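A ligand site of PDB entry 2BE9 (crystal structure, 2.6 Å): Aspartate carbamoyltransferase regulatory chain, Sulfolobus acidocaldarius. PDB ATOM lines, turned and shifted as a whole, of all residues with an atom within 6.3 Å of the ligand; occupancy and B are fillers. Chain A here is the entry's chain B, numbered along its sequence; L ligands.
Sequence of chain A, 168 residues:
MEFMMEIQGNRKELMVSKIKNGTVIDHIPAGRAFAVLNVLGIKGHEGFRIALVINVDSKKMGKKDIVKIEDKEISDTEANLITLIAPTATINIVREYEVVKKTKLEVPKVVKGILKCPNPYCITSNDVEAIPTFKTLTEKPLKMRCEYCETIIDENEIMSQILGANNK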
ATOM      1  N   VAL A  16       5.091   5.812  -5.216  1.00  0.00           N
ATOM      2  CA  VAL A  16       5.888   4.761  -4.562  1.00  0.00           C
ATOM      3  C   VAL A  16       5.311   4.390  -3.192  1.00  0.00           C
ATOM      4  O   VAL A  16       4.885   5.261  -2.430  1.00  0.00           O
ATOM      5  CB  VAL A  16       7.416   5.111  -4.462  1.00  0.00           C
ATOM      6  CG1 VAL A  16       7.691   6.116  -3.347  1.00  0.00           C
ATOM      7  CG2 VAL A  16       8.225   3.843  -4.257  1.00  0.00           C
ATOM      8  N   SER A  17       5.311   3.097  -2.900  1.00  0.00           N
ATOM      9  CA  SER A  17       4.742   2.598  -1.628  1.00  0.00           C
ATOM     10  C   SER A  17       5.389   3.248  -0.410  1.00  0.00           C
ATOM     11  O   SER A  17       6.503   3.764  -0.473  1.00  0.00           O
ATOM     12  CB  SER A  17       4.825   1.061  -1.534  1.00  0.00           C
ATOM     13  OG  SER A  17       6.038   0.622  -0.937  1.00  0.00           O
ATOM     14  N   LYS A  18       4.658   3.201   0.697  1.00  0.00           N
ATOM     15  CA  LYS A  18       5.120   3.710   1.978  1.00  0.00           C
ATOM     16  C   LYS A  18       6.303   2.888   2.521  1.00  0.00           C
ATOM     17  O   LYS A  18       6.509   1.734   2.130  1.00  0.00           O
ATOM     18  CB  LYS A  18       3.966   3.763   2.988  1.00  0.00           C
ATOM     19  CG  LYS A  18       2.662   4.454   2.497  1.00  0.00           C
ATOM     20  CD  LYS A  18       2.871   5.908   2.017  1.00  0.00           C
ATOM     21  N   ILE A  19       7.066   3.495   3.414  1.00  0.00           N
ATOM     22  CA  ILE A  19       8.312   2.923   3.893  1.00  0.00           C
ATOM     23  C   ILE A  19       8.144   2.504   5.356  1.00  0.00           C
ATOM     24  O   ILE A  19       7.517   3.205   6.144  1.00  0.00           O
ATOM     25  CB  ILE A  19       9.495   3.937   3.660  1.00  0.00           C
ATOM     26  CG1 ILE A  19      10.856   3.284   3.857  1.00  0.00           C
ATOM     27  CG2 ILE A  19       9.375   5.213   4.519  1.00  0.00           C
ATOM     28  CD1 ILE A  19      11.977   4.316   4.025  1.00  0.00           C
ATOM     29  N   LYS A  20       8.677   1.326   5.709  1.00  0.00           N
ATOM     30  CA  LYS A  20       8.550   0.845   7.072  1.00  0.00           C
ATOM     31  C   LYS A  20       9.407   1.672   8.007  1.00  0.00           C
ATOM     32  O   LYS A  20       8.911   2.222   9.004  1.00  0.00           O
ATOM     33  CB  LYS A  20       8.883  -0.648   7.186  1.00  0.00           C
ATOM     34  CG  LYS A  20       8.504  -1.273   8.540  1.00  0.00           C
ATOM     35  CD  LYS A  20       8.952  -2.743   8.667  1.00  0.00           C
ATOM     36  CE  LYS A  20       9.254  -3.102  10.127  1.00  0.00           C
ATOM     37  NZ  LYS A  20      10.325  -4.139  10.264  1.00  0.00           N
ATOM     38  N   VAL A  24      12.181  10.092   4.301  1.00  0.00           N
ATOM     39  CA  VAL A  24      11.505  10.510   3.096  1.00  0.00           C
ATOM     40  C   VAL A  24      11.800  11.964   2.894  1.00  0.00           C
ATOM     41  O   VAL A  24      11.541  12.776   3.768  1.00  0.00           O
ATOM     42  CB  VAL A  24       9.991  10.288   3.161  1.00  0.00           C
ATOM     43  CG1 VAL A  24       9.328  10.853   1.889  1.00  0.00           C
ATOM     44  CG2 VAL A  24       9.696   8.811   3.310  1.00  0.00           C
ATOM     45  N   ASP A  26      10.658  14.779   0.588  1.00  0.00           N
ATOM     46  CA  ASP A  26       9.550  15.179  -0.278  1.00  0.00           C
ATOM     47  C   ASP A  26       9.786  16.598  -0.756  1.00  0.00           C
ATOM     48  O   ASP A  26      10.684  17.286  -0.258  1.00  0.00           O
ATOM     49  CB  ASP A  26       8.250  15.122   0.517  1.00  0.00           C
ATOM     50  CG  ASP A  26       7.003  14.965  -0.356  1.00  0.00           C
ATOM     51  OD1 ASP A  26       6.997  15.241  -1.568  1.00  0.00           O
ATOM     52  OD2 ASP A  26       5.974  14.553   0.218  1.00  0.00           O
ATOM     53  N   HIS A  27       9.009  17.033  -1.735  1.00  0.00           N
ATOM     54  CA  HIS A  27       9.031  18.413  -2.225  1.00  0.00           C
ATOM     55  C   HIS A  27      10.378  18.891  -2.749  1.00  0.00           C
ATOM     56  O   HIS A  27      10.765  20.038  -2.529  1.00  0.00           O
ATOM     57  CB  HIS A  27       8.528  19.373  -1.140  1.00  0.00           C
ATOM     58  CG  HIS A  27       7.121  19.111  -0.743  1.00  0.00           C
ATOM     59  ND1 HIS A  27       6.776  18.585   0.474  1.00  0.00           N
ATOM     60  CD2 HIS A  27       5.962  19.253  -1.444  1.00  0.00           C
ATOM     61  CE1 HIS A  27       5.470  18.432   0.520  1.00  0.00           C
ATOM     62  NE2 HIS A  27       4.952  18.829  -0.623  1.00  0.00           N
ATOM     63  N   LYS A  60       1.261  22.114  -4.780  1.00  0.00           N
ATOM     64  CA  LYS A  60       1.830  23.420  -4.453  1.00  0.00           C
ATOM     65  C   LYS A  60       2.996  23.857  -5.359  1.00  0.00           C
ATOM     66  O   LYS A  60       3.264  25.056  -5.479  1.00  0.00           O
ATOM     67  CB  LYS A  60       2.224  23.494  -2.970  1.00  0.00           C
ATOM     68  CG  LYS A  60       1.058  23.869  -2.030  1.00  0.00           C
ATOM     69  CD  LYS A  60       1.495  24.017  -0.551  1.00  0.00           C
ATOM     70  CE  LYS A  60       1.372  22.697   0.238  1.00  0.00           C
ATOM     71  NZ  LYS A  60       2.310  21.610  -0.236  1.00  0.00           N
ATOM     72  N   LYS A  64       7.216  17.780  -8.783  1.00  0.00           N
ATOM     73  CA  LYS A  64       8.209  17.517  -7.760  1.00  0.00           C
ATOM     74  C   LYS A  64       8.901  16.147  -7.939  1.00  0.00           C
ATOM     75  O   LYS A  64       8.575  15.382  -8.855  1.00  0.00           O
ATOM     76  CB  LYS A  64       7.598  17.699  -6.356  1.00  0.00           C
ATOM     77  CG  LYS A  64       7.129  16.419  -5.628  1.00  0.00           C
ATOM     78  CD  LYS A  64       5.653  16.304  -5.534  1.00  0.00           C
ATOM     79  CE  LYS A  64       5.231  15.201  -4.568  1.00  0.00           C
ATOM     80  NZ  LYS A  64       4.913  15.670  -3.199  1.00  0.00           N
ATOM     81  N   ILE A  66      10.395  12.882  -5.258  1.00  0.00           N
ATOM     82  CA  ILE A  66      10.443  12.353  -3.923  1.00  0.00           C
ATOM     83  C   ILE A  66      11.545  11.309  -3.818  1.00  0.00           C
ATOM     84  O   ILE A  66      11.696  10.443  -4.698  1.00  0.00           O
ATOM     85  CB  ILE A  66       9.124  11.661  -3.526  1.00  0.00           C
ATOM     86  CG1 ILE A  66       7.917  12.606  -3.701  1.00  0.00           C
ATOM     87  CG2 ILE A  66       9.195  11.134  -2.093  1.00  0.00           C
ATOM     88  CD1 ILE A  66       6.575  11.843  -3.803  1.00  0.00           C
ATOM     89  N   LYS A  68      13.149   8.310  -1.133  1.00  0.00           N
ATOM     90  CA  LYS A  68      12.884   7.496   0.023  1.00  0.00           C
ATOM     91  C   LYS A  68      14.070   6.577   0.248  1.00  0.00           C
ATOM     92  O   LYS A  68      14.439   5.799  -0.632  1.00  0.00           O
ATOM     93  CB  LYS A  68      11.583   6.712  -0.167  1.00  0.00           C
ATOM     94  CG  LYS A  68      10.343   7.570   0.039  1.00  0.00           C
ATOM     95  CD  LYS A  68       9.095   6.802  -0.285  1.00  0.00           C
ATOM     96  CE  LYS A  68       7.872   7.692  -0.169  1.00  0.00           C
ATOM     97  NZ  LYS A  68       6.594   6.901  -0.040  1.00  0.00           N
ATOM     98  N   THR A  90      11.147  18.887   2.231  1.00  0.00           N
ATOM     99  CA  THR A  90      10.716  18.553   3.573  1.00  0.00           C
ATOM    100  C   THR A  90      11.229  17.163   3.879  1.00  0.00           C
ATOM    101  O   THR A  90      11.242  16.278   3.015  1.00  0.00           O
ATOM    102  CB  THR A  90       9.150  18.660   3.793  1.00  0.00           C
ATOM    103  OG1 THR A  90       8.450  18.095   2.689  1.00  0.00           O
ATOM    104  CG2 THR A  90       8.716  20.130   3.926  1.00  0.00           C
ATOM    105  N   ASN A  92      11.168  13.889   6.310  1.00  0.00           N
ATOM    106  CA  ASN A  92      10.397  13.120   7.249  1.00  0.00           C
ATOM    107  C   ASN A  92      11.174  11.909   7.676  1.00  0.00           C
ATOM    108  O   ASN A  92      11.674  11.165   6.847  1.00  0.00           O
ATOM    109  CB  ASN A  92       9.110  12.635   6.579  1.00  0.00           C
ATOM    110  CG  ASN A  92       8.145  13.761   6.301  1.00  0.00           C
ATOM    111  OD1 ASN A  92       8.439  14.931   6.489  1.00  0.00           O
ATOM    112  ND2 ASN A  92       6.962  13.404   5.870  1.00  0.00           N
ATOM    113  N   VAL A  94      10.873   8.299   9.322  1.00  0.00           N
ATOM    114  CA  VAL A  94       9.806   7.321   9.410  1.00  0.00           C
ATOM    115  C   VAL A  94      10.203   6.096  10.232  1.00  0.00           C
ATOM    116  O   VAL A  94      11.221   5.462   9.955  1.00  0.00           O
ATOM    117  CB  VAL A  94       9.353   6.856   8.010  1.00  0.00           C
ATOM    118  CG1 VAL A  94       8.204   5.841   8.126  1.00  0.00           C
ATOM    119  CG2 VAL A  94       8.941   8.041   7.162  1.00  0.00           C
ATOM    120  N   ARG A  95       9.384   5.784  11.242  1.00  0.00           N
ATOM    121  CA  ARG A  95       9.588   4.601  12.109  1.00  0.00           C
ATOM    122  C   ARG A  95       8.308   3.813  12.324  1.00  0.00           C
ATOM    123  O   ARG A  95       7.265   4.364  12.663  1.00  0.00           O
ATOM    124  CB  ARG A  95      10.233   5.003  13.443  1.00  0.00           C
ATOM    125  CG  ARG A  95      11.712   4.651  13.527  1.00  0.00           C
ATOM    126  CD  ARG A  95      12.556   5.803  14.044  1.00  0.00           C
ATOM    127  NE  ARG A  95      12.165   6.212  15.385  1.00  0.00           N
ATOM    128  CZ  ARG A  95      12.720   7.205  16.075  1.00  0.00           C
ATOM    129  NH1 ARG A  95      13.723   7.908  15.564  1.00  0.00           N
ATOM    130  NH2 ARG A  95      12.269   7.476  17.309  1.00  0.00           N
ATOM    131  N   GLU A  96       8.400   2.511  12.077  1.00  0.00           N
ATOM    132  CA  GLU A  96       7.279   1.574  12.205  1.00  0.00           C
ATOM    133  C   GLU A  96       6.086   1.966  11.315  1.00  0.00           C
ATOM    134  O   GLU A  96       4.967   1.519  11.550  1.00  0.00           O
ATOM    135  CB  GLU A  96       6.852   1.448  13.673  1.00  0.00           C
ATOM    136  CG  GLU A  96       6.565   0.014  14.105  1.00  0.00           C
ATOM    137  CD  GLU A  96       7.801  -0.875  14.058  1.00  0.00           C
ATOM    138  OE1 GLU A  96       7.978  -1.609  13.065  1.00  0.00           O
ATOM    139  OE2 GLU A  96       8.613  -0.810  15.017  1.00  0.00           O
ATOM    140  N   TYR A  97       6.363   2.774  10.292  1.00  0.00           N
ATOM    141  CA  TYR A  97       5.361   3.347   9.369  1.00  0.00           C
ATOM    142  C   TYR A  97       4.880   4.747   9.771  1.00  0.00           C
ATOM    143  O   TYR A  97       4.258   5.440   8.961  1.00  0.00           O
ATOM    144  CB  TYR A  97       4.164   2.404   9.122  1.00  0.00           C
ATOM    145  CG  TYR A  97       4.513   1.092   8.448  1.00  0.00           C
ATOM    146  CD1 TYR A  97       4.762  -0.053   9.204  1.00  0.00           C
ATOM    147  CD2 TYR A  97       4.565   0.996   7.055  1.00  0.00           C
ATOM    148  CE1 TYR A  97       5.076  -1.265   8.596  1.00  0.00           C
ATOM    149  CE2 TYR A  97       4.876  -0.216   6.437  1.00  0.00           C
ATOM    150  CZ  TYR A  97       5.124  -1.340   7.215  1.00  0.00           C
ATOM    151  OH  TYR A  97       5.426  -2.549   6.632  1.00  0.00           O
ATOM    152  N   GLU A  98       5.149   5.171  11.002  1.00  0.00           N
ATOM    153  CA  GLU A  98       4.737   6.502  11.454  1.00  0.00           C
ATOM    154  C   GLU A  98       5.870   7.515  11.259  1.00  0.00           C
ATOM    155  O   GLU A  98       7.034   7.253  11.598  1.00  0.00           O
ATOM    156  CB  GLU A  98       4.291   6.481  12.939  1.00  0.00           C
ATOM    157  CG  GLU A  98       3.172   5.485  13.320  1.00  0.00           C
ATOM    158  CD  GLU A  98       1.767   5.919  12.852  1.00  0.00           C
ATOM    159  OE1 GLU A  98       1.504   5.889  11.631  1.00  0.00           O
ATOM    160  OE2 GLU A  98       0.922   6.262  13.714  1.00  0.00           O
ATOM    161  N   VAL A  99       5.509   8.676  10.699  1.00  0.00           N
ATOM    162  CA  VAL A  99       6.425   9.818  10.589  1.00  0.00           C
ATOM    163  C   VAL A  99       6.670  10.366  11.998  1.00  0.00           C
ATOM    164  O   VAL A  99       5.789  10.985  12.588  1.00  0.00           O
ATOM    165  CB  VAL A  99       5.837  10.947   9.695  1.00  0.00           C
ATOM    166  CG1 VAL A  99       6.814  12.130   9.586  1.00  0.00           C
ATOM    167  CG2 VAL A  99       5.444  10.413   8.316  1.00  0.00           C
ATOM    168  N   LYS A 102       9.517  15.835  11.546  1.00  0.00           N
ATOM    169  CA  LYS A 102       9.450  16.656  10.324  1.00  0.00           C
ATOM    170  C   LYS A 102      10.417  17.840  10.407  1.00  0.00           C
ATOM    171  O   LYS A 102       9.997  18.952  10.724  1.00  0.00           O
ATOM    172  CB  LYS A 102       8.034  17.196  10.113  1.00  0.00           C
ATOM    173  CG  LYS A 102       7.072  16.217   9.478  1.00  0.00           C
ATOM    174  CD  LYS A 102       6.003  16.937   8.663  1.00  0.00           C
ATOM    175  CE  LYS A 102       5.212  15.954   7.843  1.00  0.00           C
ATOM    176  NZ  LYS A 102       4.347  15.138   8.750  1.00  0.00           N
HETATM  177  N1  LIG L   1       5.596   8.295   3.817  1.00  0.00           N
HETATM  178  C1  LIG L   1       6.174   7.061   3.583  1.00  0.00           C
HETATM  179  N2  LIG L   1       6.133   6.083   4.567  1.00  0.00           N
HETATM  180  C2  LIG L   1       5.464   6.314   5.748  1.00  0.00           C
HETATM  181  C3  LIG L   1       4.892   7.567   5.991  1.00  0.00           C
HETATM  182  C4  LIG L   1       4.833   8.476   4.936  1.00  0.00           C
HETATM  183  O1  LIG L   1       6.729   6.813   2.514  1.00  0.00           O
HETATM  184  N3  LIG L   1       5.355   5.352   6.650  1.00  0.00           N
HETATM  185  C5  LIG L   1       5.807   9.380   2.839  1.00  0.00           C
HETATM  186  C6  LIG L   1       4.485   9.876   2.237  1.00  0.00           C
HETATM  187  O2  LIG L   1       4.346   9.347   0.940  1.00  0.00           O
HETATM  188  C7  LIG L   1       4.625  11.384   2.246  1.00  0.00           C
HETATM  189  C8  LIG L   1       5.578  11.630   3.400  1.00  0.00           C
HETATM  190  O3  LIG L   1       6.435  10.518   3.420  1.00  0.00           O
HETATM  191  O4  LIG L   1       5.239  11.840   1.065  1.00  0.00           O
HETATM  192  C9  LIG L   1       4.858  11.521   4.725  1.00  0.00           C
HETATM  193  O5  LIG L   1       4.298  12.721   5.154  1.00  0.00           O
HETATM  194  P1  LIG L   1       2.912  12.585   5.925  1.00  0.00           P
HETATM  195  O6  LIG L   1       2.614  11.122   6.150  1.00  0.00           O
HETATM  196  O7  LIG L   1       2.911  13.387   7.208  1.00  0.00           O
HETATM  197  O8  LIG L   1       1.898  13.129   4.795  1.00  0.00           O
HETATM  198  P2  LIG L   1       1.671  14.705   4.635  1.00  0.00           P
HETATM  199  O9  LIG L   1       1.079  15.223   5.928  1.00  0.00           O
HETATM  200  O10 LIG L   1       0.799  15.012   3.444  1.00  0.00           O
HETATM  201  O11 LIG L   1       3.146  15.342   4.437  1.00  0.00           O
HETATM  202  P3  LIG L   1       3.408  16.923   4.236  1.00  0.00           P
HETATM  203  O12 LIG L   1       2.462  17.697   5.123  1.00  0.00           O
HETATM  204  O13 LIG L   1       3.181  17.312   2.793  1.00  0.00           O
HETATM  205  O14 LIG L   1       4.825  17.265   4.670  1.00  0.00           O
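O of Tyr 97 is in hydrogen-bond range of N3 of the ligand (2.6 Å). The side-chain amino group of Lys 102 is in salt-bridge range of an oxygen (O7) of the ligand, 2.7 Å away. An oxygen (O4) of the ligand is in hydrogen-bond range of the side-chain carboxylate of Asp 26, at 2.9 Å. The side-chain amide nitrogen of Asn 92 sits at hydrogen-bond distance from an oxygen (O5) of the ligand, at 2.8 Å. NZ of Lys 68 sits at hydrogen-bond distance from O1 of the ligand (2.6 Å). A nitrogen (N2) of the ligand is in hydrogen-bond range of the backbone NH (N) of Ile 19, 3.0 Å away. O of Ile 19 sits at hydrogen-bond distance from N3 of the ligand, at 3.1 Å.
The backbone carbonyl oxygen of Ser 17 is in hydrogen-bond range of the side-chain amino group of Lys 68, 3.2 Å away. O of Thr 90 is in hydrogen-bond range of N of Asp 26. The backbone carbonyl oxygen (O) of Lys 20 lies within hydrogen-bond range of the backbone NH (N) of Tyr 97. The side-chain carboxylate (OD1) of Asp 26 is in salt-bridge range of the side-chain amino group (NZ) of Lys 64 (2.7 Å). The side-chain hydroxyl of Thr 90 sits at hydrogen-bond distance from a ring nitrogen (ND1) of His 27, at 2.8 Å. The backbone NH (N) of Asn 92 lies within hydrogen-bond range of the backbone carbonyl oxygen (O) of Val 24 (2.8 Å). The side-chain amino group (NZ) of Lys 68 lies within hydrogen-bond range of the backbone carbonyl oxygen (O) of Val 16.
Residues that only touch the ligand: Lys 18 (3.5 Å), Val 24 (3.3 Å), His 27 (3.4 Å), Val 94 (3.2 Å) and Val 99 (3.6 Å). Hydrophobic or aromatic side chains within 4 Å of the ligand: Ile 19, Val 24, His 27, Val 94 and Val 99. Of the 21 residues printed, 11 come within 4 Å of the ligand.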
